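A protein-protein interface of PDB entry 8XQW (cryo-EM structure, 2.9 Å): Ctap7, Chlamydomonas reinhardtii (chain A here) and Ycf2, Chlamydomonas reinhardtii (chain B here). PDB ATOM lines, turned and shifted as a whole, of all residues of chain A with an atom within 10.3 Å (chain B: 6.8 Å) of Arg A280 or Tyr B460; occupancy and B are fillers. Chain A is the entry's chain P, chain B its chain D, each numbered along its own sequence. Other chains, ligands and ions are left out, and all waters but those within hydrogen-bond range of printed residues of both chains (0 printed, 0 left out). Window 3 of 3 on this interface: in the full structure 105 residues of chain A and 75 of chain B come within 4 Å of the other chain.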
ATOM      1  N   TYR A 274      -8.843  -3.159  -7.191  1.00  0.00           N
ATOM      2  CA  TYR A 274      -9.941  -2.489  -6.512  1.00  0.00           C
ATOM      3  C   TYR A 274      -9.979  -2.760  -5.018  1.00  0.00           C
ATOM      4  O   TYR A 274     -10.784  -2.146  -4.312  1.00  0.00           O
ATOM      5  CB  TYR A 274     -11.268  -2.905  -7.135  1.00  0.00           C
ATOM      6  CG  TYR A 274     -11.470  -2.432  -8.552  1.00  0.00           C
ATOM      7  CD1 TYR A 274     -11.014  -3.179  -9.625  1.00  0.00           C
ATOM      8  CD2 TYR A 274     -12.130  -1.247  -8.817  1.00  0.00           C
ATOM      9  CE1 TYR A 274     -11.210  -2.754 -10.918  1.00  0.00           C
ATOM     10  CE2 TYR A 274     -12.329  -0.813 -10.104  1.00  0.00           C
ATOM     11  CZ  TYR A 274     -11.867  -1.569 -11.151  1.00  0.00           C
ATOM     12  OH  TYR A 274     -12.062  -1.135 -12.440  1.00  0.00           O
ATOM     13  N   GLY A 276      -8.934  -2.761  -1.049  1.00  0.00           N
ATOM     14  CA  GLY A 276      -8.270  -1.912  -0.081  1.00  0.00           C
ATOM     15  C   GLY A 276      -8.746  -0.479  -0.031  1.00  0.00           C
ATOM     16  O   GLY A 276      -8.117   0.338   0.648  1.00  0.00           O
ATOM     17  N   ARG A 277      -9.829  -0.146  -0.723  1.00  0.00           N
ATOM     18  CA  ARG A 277     -10.362   1.207  -0.723  1.00  0.00           C
ATOM     19  C   ARG A 277     -11.762   1.228  -0.122  1.00  0.00           C
ATOM     20  O   ARG A 277     -12.349   0.189   0.190  1.00  0.00           O
ATOM     21  CB  ARG A 277     -10.382   1.775  -2.142  1.00  0.00           C
ATOM     22  CG  ARG A 277      -9.218   1.330  -3.013  1.00  0.00           C
ATOM     23  CD  ARG A 277      -9.308   1.977  -4.382  1.00  0.00           C
ATOM     24  NE  ARG A 277      -8.820   1.107  -5.446  1.00  0.00           N
ATOM     25  CZ  ARG A 277      -9.143   1.250  -6.728  1.00  0.00           C
ATOM     26  NH1 ARG A 277      -9.959   2.228  -7.100  1.00  0.00           N
ATOM     27  NH2 ARG A 277      -8.657   0.416  -7.637  1.00  0.00           N
ATOM     28  N   ASP A 278     -12.295   2.431   0.041  1.00  0.00           N
ATOM     29  CA  ASP A 278     -13.655   2.583   0.540  1.00  0.00           C
ATOM     30  C   ASP A 278     -14.634   1.996  -0.464  1.00  0.00           C
ATOM     31  O   ASP A 278     -14.665   2.448  -1.615  1.00  0.00           O
ATOM     32  CB  ASP A 278     -13.991   4.044   0.784  1.00  0.00           C
ATOM     33  CG  ASP A 278     -15.484   4.279   0.907  1.00  0.00           C
ATOM     34  OD1 ASP A 278     -16.143   3.535   1.660  1.00  0.00           O
ATOM     35  OD2 ASP A 278     -16.001   5.191   0.233  1.00  0.00           O
ATOM     36  N   PRO A 279     -15.455   1.016  -0.078  1.00  0.00           N
ATOM     37  CA  PRO A 279     -16.338   0.376  -1.070  1.00  0.00           C
ATOM     38  C   PRO A 279     -17.250   1.351  -1.790  1.00  0.00           C
ATOM     39  O   PRO A 279     -17.418   1.248  -3.010  1.00  0.00           O
ATOM     40  CB  PRO A 279     -17.126  -0.631  -0.221  1.00  0.00           C
ATOM     41  CG  PRO A 279     -16.272  -0.872   0.975  1.00  0.00           C
ATOM     42  CD  PRO A 279     -15.604   0.430   1.260  1.00  0.00           C
ATOM     43  N   ARG A 280     -17.840   2.306  -1.068  1.00  0.00           N
ATOM     44  CA  ARG A 280     -18.726   3.272  -1.706  1.00  0.00           C
ATOM     45  C   ARG A 280     -17.964   4.160  -2.681  1.00  0.00           C
ATOM     46  O   ARG A 280     -18.477   4.504  -3.754  1.00  0.00           O
ATOM     47  CB  ARG A 280     -19.429   4.111  -0.642  1.00  0.00           C
ATOM     48  CG  ARG A 280     -20.132   3.277   0.409  1.00  0.00           C
ATOM     49  CD  ARG A 280     -20.068   3.931   1.770  1.00  0.00           C
ATOM     50  NE  ARG A 280     -18.693   4.107   2.223  1.00  0.00           N
ATOM     51  CZ  ARG A 280     -18.352   4.689   3.367  1.00  0.00           C
ATOM     52  NH1 ARG A 280     -19.287   5.153   4.187  1.00  0.00           N
ATOM     53  NH2 ARG A 280     -17.072   4.811   3.693  1.00  0.00           N
ATOM     54  N   ALA A 281     -16.728   4.529  -2.332  1.00  0.00           N
ATOM     55  CA  ALA A 281     -15.909   5.317  -3.245  1.00  0.00           C
ATOM     56  C   ALA A 281     -15.579   4.535  -4.509  1.00  0.00           C
ATOM     57  O   ALA A 281     -15.570   5.095  -5.609  1.00  0.00           O
ATOM     58  CB  ALA A 281     -14.630   5.767  -2.547  1.00  0.00           C
ATOM     59  N   VAL A 282     -15.301   3.236  -4.373  1.00  0.00           N
ATOM     60  CA  VAL A 282     -15.042   2.416  -5.551  1.00  0.00           C
ATOM     61  C   VAL A 282     -16.309   2.240  -6.373  1.00  0.00           C
ATOM     62  O   VAL A 282     -16.252   2.132  -7.605  1.00  0.00           O
ATOM     63  CB  VAL A 282     -14.449   1.056  -5.143  1.00  0.00           C
ATOM     64  CG1 VAL A 282     -13.903   0.343  -6.356  1.00  0.00           C
ATOM     65  CG2 VAL A 282     -13.351   1.249  -4.126  1.00  0.00           C
ATOM     66  N   VAL A 283     -17.467   2.207  -5.719  1.00  0.00           N
ATOM     67  CA  VAL A 283     -18.714   2.011  -6.440  1.00  0.00           C
ATOM     68  C   VAL A 283     -19.146   3.301  -7.129  1.00  0.00           C
ATOM     69  O   VAL A 283     -19.897   3.268  -8.110  1.00  0.00           O
ATOM     70  CB  VAL A 283     -19.780   1.467  -5.468  1.00  0.00           C
ATOM     71  CG1 VAL A 283     -21.173   1.543  -6.059  1.00  0.00           C
ATOM     72  CG2 VAL A 283     -19.451   0.033  -5.097  1.00  0.00           C
ATOM     73  N   ALA A 284     -18.644   4.447  -6.666  1.00  0.00           N
ATOM     74  CA  ALA A 284     -19.085   5.725  -7.219  1.00  0.00           C
ATOM     75  C   ALA A 284     -18.658   5.921  -8.670  1.00  0.00           C
ATOM     76  O   ALA A 284     -19.321   6.656  -9.410  1.00  0.00           O
ATOM     77  CB  ALA A 284     -18.558   6.874  -6.361  1.00  0.00           C
ATOM     78  N   ASP A 285     -17.534   5.266  -9.113  1.00  0.00           N
ATOM     79  CA  ASP A 285     -17.110   5.619 -10.463  1.00  0.00           C
ATOM     80  C   ASP A 285     -17.487   4.532 -11.463  1.00  0.00           C
ATOM     81  O   ASP A 285     -17.488   3.345 -11.129  1.00  0.00           O
ATOM     82  CB  ASP A 285     -15.599   5.854 -10.518  1.00  0.00           C
ATOM     83  CG  ASP A 285     -14.804   4.633 -10.115  1.00  0.00           C
ATOM     84  OD1 ASP A 285     -14.971   4.165  -8.971  1.00  0.00           O
ATOM     85  OD2 ASP A 285     -14.012   4.138 -10.943  1.00  0.00           O
ATOM     86  N   PRO A 286     -17.799   4.915 -12.704  1.00  0.00           N
ATOM     87  CA  PRO A 286     -18.238   3.919 -13.694  1.00  0.00           C
ATOM     88  C   PRO A 286     -17.127   3.019 -14.202  1.00  0.00           C
ATOM     89  O   PRO A 286     -17.418   2.086 -14.963  1.00  0.00           O
ATOM     90  CB  PRO A 286     -18.814   4.776 -14.832  1.00  0.00           C
ATOM     91  CG  PRO A 286     -19.000   6.140 -14.247  1.00  0.00           C
ATOM     92  CD  PRO A 286     -17.923   6.283 -13.223  1.00  0.00           C
ATOM     93  N   TYR A 288     -15.377   0.886 -12.408  1.00  0.00           N
ATOM     94  CA  TYR A 288     -15.650  -0.409 -11.803  1.00  0.00           C
ATOM     95  C   TYR A 288     -16.798  -1.116 -12.513  1.00  0.00           C
ATOM     96  O   TYR A 288     -16.762  -2.337 -12.706  1.00  0.00           O
ATOM     97  CB  TYR A 288     -15.960  -0.220 -10.318  1.00  0.00           C
ATOM     98  CG  TYR A 288     -16.525  -1.431  -9.611  1.00  0.00           C
ATOM     99  CD1 TYR A 288     -17.890  -1.697  -9.622  1.00  0.00           C
ATOM    100  CD2 TYR A 288     -15.699  -2.296  -8.908  1.00  0.00           C
ATOM    101  CE1 TYR A 288     -18.409  -2.797  -8.974  1.00  0.00           C
ATOM    102  CE2 TYR A 288     -16.213  -3.399  -8.250  1.00  0.00           C
ATOM    103  CZ  TYR A 288     -17.569  -3.641  -8.289  1.00  0.00           C
ATOM    104  OH  TYR A 288     -18.089  -4.731  -7.637  1.00  0.00           O
ATOM    105  N   ARG A 503     -22.776  -6.329  -8.202  1.00  0.00           N
ATOM    106  CA  ARG A 503     -21.558  -5.530  -8.156  1.00  0.00           C
ATOM    107  C   ARG A 503     -21.103  -5.315  -6.719  1.00  0.00           C
ATOM    108  O   ARG A 503     -19.906  -5.400  -6.417  1.00  0.00           O
ATOM    109  CB  ARG A 503     -21.774  -4.196  -8.872  1.00  0.00           C
ATOM    110  CG  ARG A 503     -22.137  -4.342 -10.348  1.00  0.00           C
ATOM    111  CD  ARG A 503     -22.120  -3.016 -11.095  1.00  0.00           C
ATOM    112  NE  ARG A 503     -22.918  -3.098 -12.315  1.00  0.00           N
ATOM    113  CZ  ARG A 503     -24.109  -2.528 -12.471  1.00  0.00           C
ATOM    114  NH1 ARG A 503     -24.642  -1.820 -11.485  1.00  0.00           N
ATOM    115  NH2 ARG A 503     -24.766  -2.666 -13.613  1.00  0.00           N
ATOM    116  N   SER A 504     -22.046  -5.077  -5.808  1.00  0.00           N
ATOM    117  CA  SER A 504     -21.666  -4.824  -4.423  1.00  0.00           C
ATOM    118  C   SER A 504     -20.988  -6.039  -3.796  1.00  0.00           C
ATOM    119  O   SER A 504     -19.818  -5.983  -3.388  1.00  0.00           O
ATOM    120  CB  SER A 504     -22.896  -4.415  -3.623  1.00  0.00           C
ATOM    121  OG  SER A 504     -23.760  -3.627  -4.423  1.00  0.00           O
ATOM    122  N   LEU A 507     -17.639  -6.804  -5.141  1.00  0.00           N
ATOM    123  CA  LEU A 507     -16.592  -6.059  -4.459  1.00  0.00           C
ATOM    124  C   LEU A 507     -16.248  -6.712  -3.130  1.00  0.00           C
ATOM    125  O   LEU A 507     -15.091  -6.669  -2.699  1.00  0.00           O
ATOM    126  CB  LEU A 507     -17.034  -4.609  -4.252  1.00  0.00           C
ATOM    127  CG  LEU A 507     -16.049  -3.574  -3.700  1.00  0.00           C
ATOM    128  CD1 LEU A 507     -15.943  -3.608  -2.182  1.00  0.00           C
ATOM    129  CD2 LEU A 507     -14.684  -3.770  -4.329  1.00  0.00           C
ATOM    130  N   VAL A 508     -17.238  -7.304  -2.471  1.00  0.00           N
ATOM    131  CA  VAL A 508     -17.049  -7.876  -1.134  1.00  0.00           C
ATOM    132  C   VAL A 508     -15.858  -8.831  -1.043  1.00  0.00           C
ATOM    133  O   VAL A 508     -14.980  -8.607  -0.196  1.00  0.00           O
ATOM    134  CB  VAL A 508     -18.330  -8.568  -0.639  1.00  0.00           C
ATOM    135  CG1 VAL A 508     -17.994  -9.658   0.372  1.00  0.00           C
ATOM    136  CG2 VAL A 508     -19.242  -7.549  -0.001  1.00  0.00           C
ATOM    137  N   ASN A 511     -11.816  -8.013  -1.177  1.00  0.00           N
ATOM    138  CA  ASN A 511     -11.102  -7.531  -0.003  1.00  0.00           C
ATOM    139  C   ASN A 511     -10.552  -8.670   0.839  1.00  0.00           C
ATOM    140  O   ASN A 511     -10.206  -8.465   2.006  1.00  0.00           O
ATOM    141  CB  ASN A 511     -12.010  -6.647   0.843  1.00  0.00           C
ATOM    142  CG  ASN A 511     -12.617  -5.523   0.049  1.00  0.00           C
ATOM    143  OD1 ASN A 511     -13.188  -5.743  -1.015  1.00  0.00           O
ATOM    144  ND2 ASN A 511     -12.508  -4.306   0.565  1.00  0.00           N
ATOM    145  N   PHE A 513     -12.089 -11.582   1.855  1.00  0.00           N
ATOM    146  CA  PHE A 513     -13.088 -12.478   2.406  1.00  0.00           C
ATOM    147  C   PHE A 513     -13.847 -13.189   1.291  1.00  0.00           C
ATOM    148  O   PHE A 513     -13.455 -13.177   0.124  1.00  0.00           O
ATOM    149  CB  PHE A 513     -14.048 -11.711   3.301  1.00  0.00           C
ATOM    150  CG  PHE A 513     -13.379 -11.010   4.430  1.00  0.00           C
ATOM    151  CD1 PHE A 513     -12.972 -11.706   5.547  1.00  0.00           C
ATOM    152  CD2 PHE A 513     -13.148  -9.652   4.374  1.00  0.00           C
ATOM    153  CE1 PHE A 513     -12.356 -11.062   6.590  1.00  0.00           C
ATOM    154  CE2 PHE A 513     -12.527  -9.003   5.414  1.00  0.00           C
ATOM    155  CZ  PHE A 513     -12.130  -9.710   6.525  1.00  0.00           C
ATOM    156  N   ASN A 523     -13.969 -11.747  11.484  1.00  0.00           N
ATOM    157  CA  ASN A 523     -14.117 -10.388  10.994  1.00  0.00           C
ATOM    158  C   ASN A 523     -14.741 -10.334   9.610  1.00  0.00           C
ATOM    159  O   ASN A 523     -14.415  -9.439   8.824  1.00  0.00           O
ATOM    160  CB  ASN A 523     -12.765  -9.675  10.998  1.00  0.00           C
ATOM    161  CG  ASN A 523     -12.362  -9.208  12.383  1.00  0.00           C
ATOM    162  OD1 ASN A 523     -13.161  -8.618  13.107  1.00  0.00           O
ATOM    163  ND2 ASN A 523     -11.120  -9.475  12.762  1.00  0.00           N
ATOM    164  N   HIS A 524     -15.618 -11.270   9.290  1.00  0.00           N
ATOM    165  CA  HIS A 524     -16.360 -11.179   8.048  1.00  0.00           C
ATOM    166  C   HIS A 524     -17.339 -10.012   8.128  1.00  0.00           C
ATOM    167  O   HIS A 524     -17.928  -9.768   9.184  1.00  0.00           O
ATOM    168  CB  HIS A 524     -17.111 -12.476   7.781  1.00  0.00           C
ATOM    169  CG  HIS A 524     -17.629 -12.604   6.386  1.00  0.00           C
ATOM    170  ND1 HIS A 524     -18.857 -12.112   6.002  1.00  0.00           N
ATOM    171  CD2 HIS A 524     -17.098 -13.187   5.287  1.00  0.00           C
ATOM    172  CE1 HIS A 524     -19.056 -12.381   4.725  1.00  0.00           C
ATOM    173  NE2 HIS A 524     -18.003 -13.031   4.267  1.00  0.00           N
ATOM    174  N   PRO A 525     -17.520  -9.260   7.041  1.00  0.00           N
ATOM    175  CA  PRO A 525     -18.418  -8.103   7.112  1.00  0.00           C
ATOM    176  C   PRO A 525     -19.872  -8.479   7.303  1.00  0.00           C
ATOM    177  O   PRO A 525     -20.573  -7.808   8.069  1.00  0.00           O
ATOM    178  CB  PRO A 525     -18.189  -7.406   5.766  1.00  0.00           C
ATOM    179  CG  PRO A 525     -17.707  -8.478   4.868  1.00  0.00           C
ATOM    180  CD  PRO A 525     -16.867  -9.366   5.728  1.00  0.00           C
ATOM    181  N   LEU A 526     -20.348  -9.533   6.643  1.00  0.00           N
ATOM    182  CA  LEU A 526     -21.749  -9.931   6.722  1.00  0.00           C
ATOM    183  C   LEU A 526     -22.027 -10.835   7.915  1.00  0.00           C
ATOM    184  O   LEU A 526     -22.763 -10.458   8.829  1.00  0.00           O
ATOM    185  CB  LEU A 526     -22.159 -10.651   5.434  1.00  0.00           C
ATOM    186  CG  LEU A 526     -22.691  -9.832   4.271  1.00  0.00           C
ATOM    187  CD1 LEU A 526     -22.852 -10.723   3.061  1.00  0.00           C
ATOM    188  CD2 LEU A 526     -24.005  -9.196   4.651  1.00  0.00           C
ATOM    189  N   PRO A 654      -5.474  -6.840   3.822  1.00  0.00           N
ATOM    190  CA  PRO A 654      -6.537  -7.844   3.932  1.00  0.00           C
ATOM    191  C   PRO A 654      -6.929  -8.496   2.619  1.00  0.00           C
ATOM    192  O   PRO A 654      -7.764  -9.407   2.634  1.00  0.00           O
ATOM    193  CB  PRO A 654      -7.705  -7.036   4.499  1.00  0.00           C
ATOM    194  CG  PRO A 654      -7.494  -5.678   3.933  1.00  0.00           C
ATOM    195  CD  PRO A 654      -6.005  -5.468   3.863  1.00  0.00           C
ATOM    196  N   CYS B 455     -23.038  -4.300   5.287  1.00  0.00           N
ATOM    197  CA  CYS B 455     -21.795  -4.902   4.829  1.00  0.00           C
ATOM    198  C   CYS B 455     -20.776  -3.836   4.465  1.00  0.00           C
ATOM    199  O   CYS B 455     -19.611  -3.910   4.869  1.00  0.00           O
ATOM    200  CB  CYS B 455     -22.067  -5.810   3.632  1.00  0.00           C
ATOM    201  SG  CYS B 455     -20.785  -7.034   3.329  1.00  0.00           S
ATOM    202  N   PHE B 456     -21.198  -2.833   3.698  1.00  0.00           N
ATOM    203  CA  PHE B 456     -20.258  -1.811   3.257  1.00  0.00           C
ATOM    204  C   PHE B 456     -19.798  -0.947   4.420  1.00  0.00           C
ATOM    205  O   PHE B 456     -18.620  -0.570   4.493  1.00  0.00           O
ATOM    206  CB  PHE B 456     -20.888  -0.965   2.159  1.00  0.00           C
ATOM    207  CG  PHE B 456     -20.713  -1.541   0.789  1.00  0.00           C
ATOM    208  CD1 PHE B 456     -19.973  -2.694   0.607  1.00  0.00           C
ATOM    209  CD2 PHE B 456     -21.282  -0.937  -0.312  1.00  0.00           C
ATOM    210  CE1 PHE B 456     -19.801  -3.234  -0.648  1.00  0.00           C
ATOM    211  CE2 PHE B 456     -21.114  -1.471  -1.570  1.00  0.00           C
ATOM    212  CZ  PHE B 456     -20.372  -2.622  -1.739  1.00  0.00           C
ATOM    213  N   ASN B 457     -20.703  -0.642   5.352  1.00  0.00           N
ATOM    214  CA  ASN B 457     -20.299   0.062   6.565  1.00  0.00           C
ATOM    215  C   ASN B 457     -19.197  -0.695   7.291  1.00  0.00           C
ATOM    216  O   ASN B 457     -18.139  -0.134   7.600  1.00  0.00           O
ATOM    217  CB  ASN B 457     -21.498   0.260   7.488  1.00  0.00           C
ATOM    218  CG  ASN B 457     -22.633   0.993   6.819  1.00  0.00           C
ATOM    219  OD1 ASN B 457     -23.801   0.673   7.032  1.00  0.00           O
ATOM    220  ND2 ASN B 457     -22.297   1.978   6.000  1.00  0.00           N
ATOM    221  N   ASN B 458     -19.431  -1.980   7.569  1.00  0.00           N
ATOM    222  CA  ASN B 458     -18.455  -2.756   8.324  1.00  0.00           C
ATOM    223  C   ASN B 458     -17.155  -2.919   7.552  1.00  0.00           C
ATOM    224  O   ASN B 458     -16.071  -2.914   8.143  1.00  0.00           O
ATOM    225  CB  ASN B 458     -19.037  -4.117   8.690  1.00  0.00           C
ATOM    226  CG  ASN B 458     -19.999  -4.040   9.850  1.00  0.00           C
ATOM    227  OD1 ASN B 458     -19.606  -4.178  11.005  1.00  0.00           O
ATOM    228  ND2 ASN B 458     -21.270  -3.812   9.547  1.00  0.00           N
ATOM    229  N   LEU B 459     -17.237  -3.053   6.229  1.00  0.00           N
ATOM    230  CA  LEU B 459     -16.024  -3.200   5.437  1.00  0.00           C
ATOM    231  C   LEU B 459     -15.175  -1.941   5.502  1.00  0.00           C
ATOM    232  O   LEU B 459     -13.951  -2.015   5.679  1.00  0.00           O
ATOM    233  CB  LEU B 459     -16.382  -3.531   3.990  1.00  0.00           C
ATOM    234  CG  LEU B 459     -15.222  -3.878   3.061  1.00  0.00           C
ATOM    235  CD1 LEU B 459     -14.275  -4.849   3.738  1.00  0.00           C
ATOM    236  CD2 LEU B 459     -15.745  -4.464   1.766  1.00  0.00           C
ATOM    237  N   TYR B 460     -15.806  -0.775   5.355  1.00  0.00           N
ATOM    238  CA  TYR B 460     -15.058   0.471   5.454  1.00  0.00           C
ATOM    239  C   TYR B 460     -14.453   0.631   6.841  1.00  0.00           C
ATOM    240  O   TYR B 460     -13.302   1.059   6.979  1.00  0.00           O
ATOM    241  CB  TYR B 460     -15.956   1.658   5.121  1.00  0.00           C
ATOM    242  CG  TYR B 460     -15.276   2.981   5.361  1.00  0.00           C
ATOM    243  CD1 TYR B 460     -14.280   3.434   4.505  1.00  0.00           C
ATOM    244  CD2 TYR B 460     -15.615   3.772   6.449  1.00  0.00           C
ATOM    245  CE1 TYR B 460     -13.652   4.642   4.723  1.00  0.00           C
ATOM    246  CE2 TYR B 460     -14.993   4.977   6.674  1.00  0.00           C
ATOM    247  CZ  TYR B 460     -14.011   5.407   5.810  1.00  0.00           C
ATOM    248  OH  TYR B 460     -13.388   6.614   6.034  1.00  0.00           O
ATOM    249  N   ASN B 461     -15.221   0.305   7.883  1.00  0.00           N
ATOM    250  CA  ASN B 461     -14.679   0.378   9.236  1.00  0.00           C
ATOM    251  C   ASN B 461     -13.468  -0.528   9.381  1.00  0.00           C
ATOM    252  O   ASN B 461     -12.468  -0.158  10.002  1.00  0.00           O
ATOM    253  CB  ASN B 461     -15.749   0.004  10.259  1.00  0.00           C
ATOM    254  CG  ASN B 461     -16.994   0.838  10.122  1.00  0.00           C
ATOM    255  OD1 ASN B 461     -18.097   0.380  10.415  1.00  0.00           O
ATOM    256  ND2 ASN B 461     -16.831   2.071   9.661  1.00  0.00           N
ATOM    257  N   TYR B 462     -13.544  -1.723   8.798  1.00  0.00           N
ATOM    258  CA  TYR B 462     -12.439  -2.671   8.853  1.00  0.00           C
ATOM    259  C   TYR B 462     -11.182  -2.083   8.225  1.00  0.00           C
ATOM    260  O   TYR B 462     -10.118  -2.016   8.861  1.00  0.00           O
ATOM    261  CB  TYR B 462     -12.863  -3.949   8.132  1.00  0.00           C
ATOM    262  CG  TYR B 462     -11.990  -5.147   8.359  1.00  0.00           C
ATOM    263  CD1 TYR B 462     -11.864  -5.704   9.618  1.00  0.00           C
ATOM    264  CD2 TYR B 462     -11.315  -5.739   7.307  1.00  0.00           C
ATOM    265  CE1 TYR B 462     -11.079  -6.809   9.824  1.00  0.00           C
ATOM    266  CE2 TYR B 462     -10.524  -6.840   7.503  1.00  0.00           C
ATOM    267  CZ  TYR B 462     -10.408  -7.372   8.764  1.00  0.00           C
ATOM    268  OH  TYR B 462      -9.616  -8.478   8.968  1.00  0.00           O
ATOM    269  N   ILE B 463     -11.297  -1.644   6.970  1.00  0.00           N
ATOM    270  CA  ILE B 463     -10.155  -1.064   6.269  1.00  0.00           C
ATOM    271  C   ILE B 463      -9.581   0.102   7.063  1.00  0.00           C
ATOM    272  O   ILE B 463      -8.368   0.183   7.291  1.00  0.00           O
ATOM    273  CB  ILE B 463     -10.560  -0.620   4.850  1.00  0.00           C
ATOM    274  CG1 ILE B 463     -11.222  -1.767   4.085  1.00  0.00           C
ATOM    275  CG2 ILE B 463      -9.352  -0.094   4.103  1.00  0.00           C
ATOM    276  CD1 ILE B 463     -10.336  -2.971   3.884  1.00  0.00           C
ATOM    277  N   SER B 464     -10.447   1.019   7.498  1.00  0.00           N
ATOM    278  CA  SER B 464      -9.973   2.235   8.144  1.00  0.00           C
ATOM    279  C   SER B 464      -9.300   1.934   9.475  1.00  0.00           C
ATOM    280  O   SER B 464      -8.244   2.501   9.780  1.00  0.00           O
ATOM    281  CB  SER B 464     -11.130   3.213   8.333  1.00  0.00           C
ATOM    282  OG  SER B 464     -11.938   3.280   7.171  1.00  0.00           O
ATOM    283  N   ASN B 465      -9.891   1.052  10.282  1.00  0.00           N
ATOM    284  CA  ASN B 465      -9.295   0.723  11.570  1.00  0.00           C
ATOM    285  C   ASN B 465      -7.929   0.082  11.389  1.00  0.00           C
ATOM    286  O   ASN B 465      -6.982   0.409  12.115  1.00  0.00           O
ATOM    287  CB  ASN B 465     -10.218  -0.201  12.360  1.00  0.00           C
ATOM    288  CG  ASN B 465      -9.999  -0.092  13.853  1.00  0.00           C
ATOM    289  OD1 ASN B 465      -8.884   0.164  14.307  1.00  0.00           O
ATOM    290  ND2 ASN B 465     -11.061  -0.274  14.626  1.00  0.00           N
ATOM    291  N   LYS B 466      -7.796  -0.818  10.411  1.00  0.00           N
ATOM    292  CA  LYS B 466      -6.500  -1.456  10.216  1.00  0.00           C
ATOM    293  C   LYS B 466      -5.460  -0.476   9.691  1.00  0.00           C
ATOM    294  O   LYS B 466      -4.303  -0.508  10.118  1.00  0.00           O
ATOM    295  CB  LYS B 466      -6.625  -2.672   9.305  1.00  0.00           C
ATOM    296  CG  LYS B 466      -6.686  -3.938  10.120  1.00  0.00           C
ATOM    297  CD  LYS B 466      -7.635  -4.973   9.588  1.00  0.00           C
ATOM    298  CE  LYS B 466      -7.975  -5.936  10.719  1.00  0.00           C
ATOM    299  NZ  LYS B 466      -7.846  -7.370  10.322  1.00  0.00           N
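O of Asn A511 lies close to O of Pro A654 (2.7 Å). O of Tyr B460 sits at hydrogen-bond distance from OG of Ser B464. OD1 of Asn A511 lies close to O of Leu A507 (2.7 Å). OD1 of Asp A278 is in salt-bridge range of NH2 of Arg A280 (2.6 Å). ND1 of His A524 is in hydrogen-bond range of N of Leu A526, at 3.0 Å. NZ of Lys B466 sits at hydrogen-bond distance from OH of Tyr B462.
Among the printed residues, pairs that only touch across the chains: Gly A276 with Ile B463, Asp A278 with Tyr B460, Pro A279 with Phe B456, Pro A279 with Leu B459, Arg A280 with Tyr B460, Ser A504 with Phe B456, Val A508 with Cys B455, Asn A511 with Leu B459, Phe A513 with Tyr B462, Asn A523 with Tyr B462, Pro A525 with Cys B455, Leu A526 with Cys B455 and Pro A654 with Ile B463.
Arg A280 touches just one residue of chain B: Tyr B460 (3.1 Å). Of the printed residues of chain A, Tyr B460 touches Asp A278 (3.4 Å) and Arg A280 (3.1 Å). Of chain A, only Pro A279 and Ser A504 come within 4 Å of Phe B456. No residue of chain A comes within 4 Å of Asn B461. Ile B463 touches just these residues of chain A: Gly A276 (3.7 Å) and Pro A654 (3.9 Å). No residue of chain A comes within 4 Å of Ser B464. Printed residues of chain B within 4 Å of Val A508: Cys B455 (3.7 Å). Printed residues of chain B within 4 Å of Pro A654: Ile B463. His A524 touches none of the printed residues of chain B. Lys B466 touches none of the printed residues of chain A. The nearest residue of chain A that does not touch Tyr B460 is Pro A279 (4.1 Å). The nearest printed residue of chain B that does not touch Ser A504 is Leu B459 (6.7 Å).
Hydrophobic or aromatic side chains of chain A within 4 Å of the printed part of chain B: Pro A279, Val A508, Phe A513, Pro A525, Leu A526 and Pro A654. Hydrophobic or aromatic side chains of chain B within 4 Å of the printed part of chain A: Phe B456, Leu B459, Tyr B460, Tyr B462 and Ile B463. Among the printed residues, 13 pairs touch across the chains. Among the printed residues, no Asp or Glu carboxylate lies within 4 Å of a Lys or Arg side-chain nitrogen of the other chain.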
